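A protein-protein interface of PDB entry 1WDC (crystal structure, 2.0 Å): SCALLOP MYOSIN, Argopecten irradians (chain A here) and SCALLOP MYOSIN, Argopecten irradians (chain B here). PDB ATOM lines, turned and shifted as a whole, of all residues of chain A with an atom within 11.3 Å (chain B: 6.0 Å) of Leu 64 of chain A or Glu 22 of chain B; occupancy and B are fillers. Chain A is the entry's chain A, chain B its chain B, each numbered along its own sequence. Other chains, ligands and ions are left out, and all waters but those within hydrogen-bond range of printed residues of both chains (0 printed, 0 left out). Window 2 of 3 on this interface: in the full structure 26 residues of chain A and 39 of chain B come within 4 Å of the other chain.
Of the printed residues of chain B, Leu 56 of chain A touches Ile 27.
Lys 59 of chain A touches none of the printed residues of chain B.
Of the printed residues of chain B, Val 60 of chain A touches Met 26 (3.6 Å).
Printed residues of chain B within 4 Å of Leu 63 of chain A: Met 26 (3.5 Å).
Of chain B, only Glu 22 (3.4 Å) and Ala 23 (3.9 Å) come within 4 Å of Leu 64 of chain A.
Of the printed residues of chain A, Met 20 of chain B touches Tyr 57.
No residue of chain A comes within 4 Å of Lys 21 of chain B.
Glu 22 of chain B touches just one residue of chain A: Leu 64.
Ala 23 of chain B touches just these residues of chain A: Tyr 57 (3.5 Å) and Leu 64 (3.9 Å).
No residue of chain A comes within 4 Å of Ser 25 of chain B.
Of the printed residues of chain A, Ile 27 of chain B touches Leu 56 (3.8 Å).
The nearest residue of chain B that does not touch Leu 64 of chain A is Met 26 of chain B (4.1 Å).
The nearest residue of chain A that does not touch Glu 22 of chain B is Val 60 of chain A (5.1 Å).
OE1 of Glu 19 of chain B sits at hydrogen-bond distance from OH of Tyr 57 of chain A (3.2 Å).
OXT of Leu 64 of chain A sits close to OE2 of Glu 22 of chain B (3.4 Å).
The side-chain hydroxyl (OG) of Ser 25 of chain B lies within hydrogen-bond range of the backbone carbonyl oxygen (O) of Glu 22 of chain B (3.4 Å).
Printed residues of chain B that touch a printed residue of chain A: Glu 19, Met 20, Glu 22, Ala 23, Met 26 and Ile 27.
Hydrophobic or aromatic side chains of chain A within 4 Å of the printed part of chain B: Leu 56, Tyr 57, Val 60, Leu 63 and Leu 64.
Among the printed residues, no Asp or Glu carboxylate lies within 4 Å of a Lys or Arg side-chain nitrogen of the other chain.
Leu 56 of chain A touches Ile 27 of chain B.
Tyr 57 of chain A touches Met 20 of chain B (OH to CE, 3.9 Å).
Ala 23 of chain B touches Tyr 57 of chain A.
Met 26 of chain B touches Val 60 of chain A.
Met 26 of chain B touches Leu 63 of chain A (CE to CD1, 3.5 Å).
Leu 64 of chain A touches Ala 23 of chain B (CD2 to N, 3.9 Å).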
ATOM      1  N   TRP A  54      -4.208  -0.567  11.207  1.00  0.00           N
ATOM      2  CA  TRP A  54      -5.422  -1.111  11.833  1.00  0.00           C
ATOM      3  C   TRP A  54      -5.791  -0.325  13.068  1.00  0.00           C
ATOM      4  O   TRP A  54      -6.952   0.073  13.218  1.00  0.00           O
ATOM      5  CB  TRP A  54      -5.228  -2.574  12.242  1.00  0.00           C
ATOM      6  CG  TRP A  54      -6.553  -3.249  12.507  1.00  0.00           C
ATOM      7  CD1 TRP A  54      -7.084  -3.594  13.743  1.00  0.00           C
ATOM      8  CD2 TRP A  54      -7.636  -3.353  11.567  1.00  0.00           C
ATOM      9  NE1 TRP A  54      -8.440  -3.835  13.621  1.00  0.00           N
ATOM     10  CE2 TRP A  54      -8.806  -3.675  12.304  1.00  0.00           C
ATOM     11  CE3 TRP A  54      -7.739  -3.156  10.176  1.00  0.00           C
ATOM     12  CZ2 TRP A  54     -10.059  -3.779  11.696  1.00  0.00           C
ATOM     13  CZ3 TRP A  54      -8.987  -3.264   9.568  1.00  0.00           C
ATOM     14  CH2 TRP A  54     -10.130  -3.567  10.328  1.00  0.00           C
ATOM     15  N   LEU A  56      -4.981   2.628  13.709  1.00  0.00           N
ATOM     16  CA  LEU A  56      -5.459   3.943  13.314  1.00  0.00           C
ATOM     17  C   LEU A  56      -6.886   3.835  12.772  1.00  0.00           C
ATOM     18  O   LEU A  56      -7.791   4.481  13.288  1.00  0.00           O
ATOM     19  CB  LEU A  56      -4.527   4.600  12.280  1.00  0.00           C
ATOM     20  CG  LEU A  56      -5.084   5.852  11.576  1.00  0.00           C
ATOM     21  CD1 LEU A  56      -5.347   6.981  12.576  1.00  0.00           C
ATOM     22  CD2 LEU A  56      -4.097   6.311  10.525  1.00  0.00           C
ATOM     23  N   TYR A  57      -7.101   3.005  11.756  1.00  0.00           N
ATOM     24  CA  TYR A  57      -8.444   2.818  11.240  1.00  0.00           C
ATOM     25  C   TYR A  57      -9.467   2.532  12.338  1.00  0.00           C
ATOM     26  O   TYR A  57     -10.588   3.017  12.277  1.00  0.00           O
ATOM     27  CB  TYR A  57      -8.461   1.682  10.221  1.00  0.00           C
ATOM     28  CG  TYR A  57      -9.835   1.432   9.613  1.00  0.00           C
ATOM     29  CD1 TYR A  57     -10.346   2.275   8.619  1.00  0.00           C
ATOM     30  CD2 TYR A  57     -10.573   0.297   9.956  1.00  0.00           C
ATOM     31  CE1 TYR A  57     -11.545   1.979   7.974  1.00  0.00           C
ATOM     32  CE2 TYR A  57     -11.769  -0.008   9.307  1.00  0.00           C
ATOM     33  CZ  TYR A  57     -12.241   0.831   8.310  1.00  0.00           C
ATOM     34  OH  TYR A  57     -13.329   0.447   7.563  1.00  0.00           O
ATOM     35  N   SER A  58      -9.078   1.760  13.346  1.00  0.00           N
ATOM     36  CA  SER A  58     -10.010   1.371  14.395  1.00  0.00           C
ATOM     37  C   SER A  58     -10.485   2.516  15.284  1.00  0.00           C
ATOM     38  O   SER A  58     -11.639   2.518  15.681  1.00  0.00           O
ATOM     39  CB  SER A  58      -9.417   0.264  15.261  1.00  0.00           C
ATOM     40  OG  SER A  58      -9.207  -0.911  14.495  1.00  0.00           O
ATOM     41  N   LYS A  59      -9.670   3.561  15.450  1.00  0.00           N
ATOM     42  CA  LYS A  59     -10.071   4.761  16.208  1.00  0.00           C
ATOM     43  C   LYS A  59     -10.916   5.783  15.433  1.00  0.00           C
ATOM     44  O   LYS A  59     -11.587   6.625  16.033  1.00  0.00           O
ATOM     45  CB  LYS A  59      -8.831   5.455  16.753  1.00  0.00           C
ATOM     46  CG  LYS A  59      -7.986   4.578  17.602  1.00  0.00           C
ATOM     47  CD  LYS A  59      -6.600   5.129  17.683  1.00  0.00           C
ATOM     48  CE  LYS A  59      -6.002   4.830  19.022  1.00  0.00           C
ATOM     49  NZ  LYS A  59      -6.782   5.462  20.126  1.00  0.00           N
ATOM     50  N   VAL A  60     -10.784   5.769  14.109  1.00  0.00           N
ATOM     51  CA  VAL A  60     -11.520   6.659  13.202  1.00  0.00           C
ATOM     52  C   VAL A  60     -12.798   5.919  12.740  1.00  0.00           C
ATOM     53  O   VAL A  60     -13.680   6.509  12.116  1.00  0.00           O
ATOM     54  CB  VAL A  60     -10.628   7.049  11.919  1.00  0.00           C
ATOM     55  CG1 VAL A  60     -11.344   8.073  11.017  1.00  0.00           C
ATOM     56  CG2 VAL A  60      -9.289   7.619  12.340  1.00  0.00           C
ATOM     57  N   LYS A  61     -12.888   4.625  13.038  1.00  0.00           N
ATOM     58  CA  LYS A  61     -14.085   3.850  12.710  1.00  0.00           C
ATOM     59  C   LYS A  61     -15.370   4.403  13.329  1.00  0.00           C
ATOM     60  O   LYS A  61     -16.385   4.519  12.643  1.00  0.00           O
ATOM     61  CB  LYS A  61     -13.911   2.381  13.112  1.00  0.00           C
ATOM     62  CG  LYS A  61     -13.677   1.466  11.947  1.00  0.00           C
ATOM     63  CD  LYS A  61     -14.943   1.249  11.178  1.00  0.00           C
ATOM     64  CE  LYS A  61     -15.613  -0.044  11.612  1.00  0.00           C
ATOM     65  NZ  LYS A  61     -14.748  -1.263  11.443  1.00  0.00           N
ATOM     66  N   PRO A  62     -15.332   4.796  14.619  1.00  0.00           N
ATOM     67  CA  PRO A  62     -16.450   5.439  15.325  1.00  0.00           C
ATOM     68  C   PRO A  62     -16.921   6.816  14.827  1.00  0.00           C
ATOM     69  O   PRO A  62     -18.116   7.065  14.727  1.00  0.00           O
ATOM     70  CB  PRO A  62     -15.941   5.520  16.761  1.00  0.00           C
ATOM     71  CG  PRO A  62     -15.035   4.357  16.875  1.00  0.00           C
ATOM     72  CD  PRO A  62     -14.302   4.351  15.574  1.00  0.00           C
ATOM     73  N   LEU A  63     -15.979   7.710  14.556  1.00  0.00           N
ATOM     74  CA  LEU A  63     -16.291   9.101  14.242  1.00  0.00           C
ATOM     75  C   LEU A  63     -17.067   9.281  12.955  1.00  0.00           C
ATOM     76  O   LEU A  63     -17.586  10.365  12.696  1.00  0.00           O
ATOM     77  CB  LEU A  63     -15.014   9.924  14.129  1.00  0.00           C
ATOM     78  CG  LEU A  63     -13.909   9.787  15.178  1.00  0.00           C
ATOM     79  CD1 LEU A  63     -13.238  11.153  15.290  1.00  0.00           C
ATOM     80  CD2 LEU A  63     -14.446   9.297  16.551  1.00  0.00           C
ATOM     81  N   LEU A  64     -17.054   8.259  12.108  1.00  0.00           N
ATOM     82  CA  LEU A  64     -17.622   8.366  10.768  1.00  0.00           C
ATOM     83  C   LEU A  64     -19.157   8.535  10.767  1.00  0.00           C
ATOM     84  O   LEU A  64     -19.803   8.326  11.831  1.00  0.00           O
ATOM     85  CB  LEU A  64     -17.223   7.144   9.938  1.00  0.00           C
ATOM     86  CG  LEU A  64     -15.799   6.640  10.110  1.00  0.00           C
ATOM     87  CD1 LEU A  64     -15.674   5.279   9.509  1.00  0.00           C
ATOM     88  CD2 LEU A  64     -14.837   7.584   9.461  1.00  0.00           C
ATOM     89  OXT LEU A  64     -19.695   8.954   9.709  1.00  0.00           O
ATOM     90  N   ILE B  17     -15.090  -1.120   1.090  1.00  0.00           N
ATOM     91  CA  ILE B  17     -14.303  -0.237   0.265  1.00  0.00           C
ATOM     92  C   ILE B  17     -14.842   1.173   0.469  1.00  0.00           C
ATOM     93  O   ILE B  17     -14.073   2.113   0.628  1.00  0.00           O
ATOM     94  CB  ILE B  17     -14.367  -0.672  -1.249  1.00  0.00           C
ATOM     95  CG1 ILE B  17     -13.195  -1.613  -1.583  1.00  0.00           C
ATOM     96  CG2 ILE B  17     -14.307   0.533  -2.186  1.00  0.00           C
ATOM     97  CD1 ILE B  17     -13.022  -1.926  -3.086  1.00  0.00           C
ATOM     98  N   GLN B  18     -16.146   1.277   0.699  1.00  0.00           N
ATOM     99  CA  GLN B  18     -16.794   2.573   0.840  1.00  0.00           C
ATOM    100  C   GLN B  18     -16.512   3.181   2.214  1.00  0.00           C
ATOM    101  O   GLN B  18     -16.396   4.406   2.332  1.00  0.00           O
ATOM    102  CB  GLN B  18     -18.306   2.432   0.604  1.00  0.00           C
ATOM    103  CG  GLN B  18     -19.194   3.410   1.391  1.00  0.00           C
ATOM    104  CD  GLN B  18     -20.354   2.714   2.106  1.00  0.00           C
ATOM    105  OE1 GLN B  18     -21.503   2.756   1.638  1.00  0.00           O
ATOM    106  NE2 GLN B  18     -20.057   2.062   3.238  1.00  0.00           N
ATOM    107  N   GLU B  19     -16.369   2.321   3.230  1.00  0.00           N
ATOM    108  CA  GLU B  19     -16.027   2.727   4.603  1.00  0.00           C
ATOM    109  C   GLU B  19     -14.637   3.338   4.726  1.00  0.00           C
ATOM    110  O   GLU B  19     -14.403   4.133   5.635  1.00  0.00           O
ATOM    111  CB  GLU B  19     -16.042   1.530   5.525  1.00  0.00           C
ATOM    112  CG  GLU B  19     -17.344   1.235   6.184  1.00  0.00           C
ATOM    113  CD  GLU B  19     -17.369  -0.183   6.737  1.00  0.00           C
ATOM    114  OE1 GLU B  19     -16.297  -0.712   7.140  1.00  0.00           O
ATOM    115  OE2 GLU B  19     -18.459  -0.794   6.706  1.00  0.00           O
ATOM    116  N   MET B  20     -13.689   2.798   3.949  1.00  0.00           N
ATOM    117  CA  MET B  20     -12.275   3.225   3.940  1.00  0.00           C
ATOM    118  C   MET B  20     -12.029   4.595   3.296  1.00  0.00           C
ATOM    119  O   MET B  20     -11.057   5.280   3.614  1.00  0.00           O
ATOM    120  CB  MET B  20     -11.422   2.184   3.227  1.00  0.00           C
ATOM    121  CG  MET B  20     -11.645   0.788   3.725  1.00  0.00           C
ATOM    122  SD  MET B  20     -10.110  -0.054   3.980  1.00  0.00           S
ATOM    123  CE  MET B  20     -10.540  -1.092   5.379  1.00  0.00           C
ATOM    124  N   LYS B  21     -12.816   4.877   2.270  1.00  0.00           N
ATOM    125  CA  LYS B  21     -12.936   6.193   1.683  1.00  0.00           C
ATOM    126  C   LYS B  21     -13.217   7.260   2.738  1.00  0.00           C
ATOM    127  O   LYS B  21     -12.666   8.342   2.678  1.00  0.00           O
ATOM    128  CB  LYS B  21     -14.073   6.158   0.659  1.00  0.00           C
ATOM    129  CG  LYS B  21     -13.676   6.566  -0.736  1.00  0.00           C
ATOM    130  CD  LYS B  21     -13.616   8.084  -0.844  1.00  0.00           C
ATOM    131  CE  LYS B  21     -12.450   8.525  -1.729  1.00  0.00           C
ATOM    132  NZ  LYS B  21     -11.131   8.197  -1.108  1.00  0.00           N
ATOM    133  N   GLU B  22     -14.129   6.976   3.660  1.00  0.00           N
ATOM    134  CA  GLU B  22     -14.522   7.942   4.684  1.00  0.00           C
ATOM    135  C   GLU B  22     -13.480   8.012   5.784  1.00  0.00           C
ATOM    136  O   GLU B  22     -13.308   9.050   6.404  1.00  0.00           O
ATOM    137  CB  GLU B  22     -15.878   7.568   5.305  1.00  0.00           C
ATOM    138  CG  GLU B  22     -16.973   8.651   5.177  1.00  0.00           C
ATOM    139  CD  GLU B  22     -16.836   9.831   6.177  1.00  0.00           C
ATOM    140  OE1 GLU B  22     -15.909  10.671   6.000  1.00  0.00           O
ATOM    141  OE2 GLU B  22     -17.712   9.969   7.083  1.00  0.00           O
ATOM    142  N   ALA B  23     -12.901   6.863   6.117  1.00  0.00           N
ATOM    143  CA  ALA B  23     -11.792   6.813   7.056  1.00  0.00           C
ATOM    144  C   ALA B  23     -10.646   7.602   6.442  1.00  0.00           C
ATOM    145  O   ALA B  23     -10.080   8.476   7.095  1.00  0.00           O
ATOM    146  CB  ALA B  23     -11.359   5.368   7.303  1.00  0.00           C
ATOM    147  N   PHE B  24     -10.430   7.405   5.142  1.00  0.00           N
ATOM    148  CA  PHE B  24      -9.318   8.037   4.458  1.00  0.00           C
ATOM    149  C   PHE B  24      -9.397   9.571   4.403  1.00  0.00           C
ATOM    150  O   PHE B  24      -8.366  10.253   4.423  1.00  0.00           O
ATOM    151  CB  PHE B  24      -9.180   7.478   3.037  1.00  0.00           C
ATOM    152  CG  PHE B  24      -8.097   8.134   2.243  1.00  0.00           C
ATOM    153  CD1 PHE B  24      -8.342   9.336   1.577  1.00  0.00           C
ATOM    154  CD2 PHE B  24      -6.788   7.640   2.302  1.00  0.00           C
ATOM    155  CE1 PHE B  24      -7.296  10.056   1.008  1.00  0.00           C
ATOM    156  CE2 PHE B  24      -5.721   8.345   1.731  1.00  0.00           C
ATOM    157  CZ  PHE B  24      -5.975   9.563   1.089  1.00  0.00           C
ATOM    158  N   SER B  25     -10.605  10.113   4.269  1.00  0.00           N
ATOM    159  CA  SER B  25     -10.781  11.563   4.176  1.00  0.00           C
ATOM    160  C   SER B  25     -10.862  12.291   5.538  1.00  0.00           C
ATOM    161  O   SER B  25     -10.948  13.524   5.607  1.00  0.00           O
ATOM    162  CB  SER B  25     -12.012  11.871   3.313  1.00  0.00           C
ATOM    163  OG  SER B  25     -13.155  11.197   3.800  1.00  0.00           O
ATOM    164  N   MET B  26     -10.745  11.526   6.617  1.00  0.00           N
ATOM    165  CA  MET B  26     -10.589  12.074   7.962  1.00  0.00           C
ATOM    166  C   MET B  26      -9.128  11.987   8.377  1.00  0.00           C
ATOM    167  O   MET B  26      -8.661  12.784   9.201  1.00  0.00           O
ATOM    168  CB  MET B  26     -11.417  11.263   8.945  1.00  0.00           C
ATOM    169  CG  MET B  26     -12.691  11.916   9.365  1.00  0.00           C
ATOM    170  SD  MET B  26     -13.226  11.102  10.848  1.00  0.00           S
ATOM    171  CE  MET B  26     -12.097  11.833  12.101  1.00  0.00           C
ATOM    172  N   ILE B  27      -8.480  10.900   7.954  1.00  0.00           N
ATOM    173  CA  ILE B  27      -7.039  10.749   8.112  1.00  0.00           C
ATOM    174  C   ILE B  27      -6.330  11.781   7.234  1.00  0.00           C
ATOM    175  O   ILE B  27      -5.295  12.308   7.622  1.00  0.00           O
ATOM    176  CB  ILE B  27      -6.564   9.343   7.699  1.00  0.00           C
ATOM    177  CG1 ILE B  27      -7.314   8.284   8.511  1.00  0.00           C
ATOM    178  CG2 ILE B  27      -5.057   9.205   7.908  1.00  0.00           C
ATOM    179  CD1 ILE B  27      -6.934   6.837   8.129  1.00  0.00           C
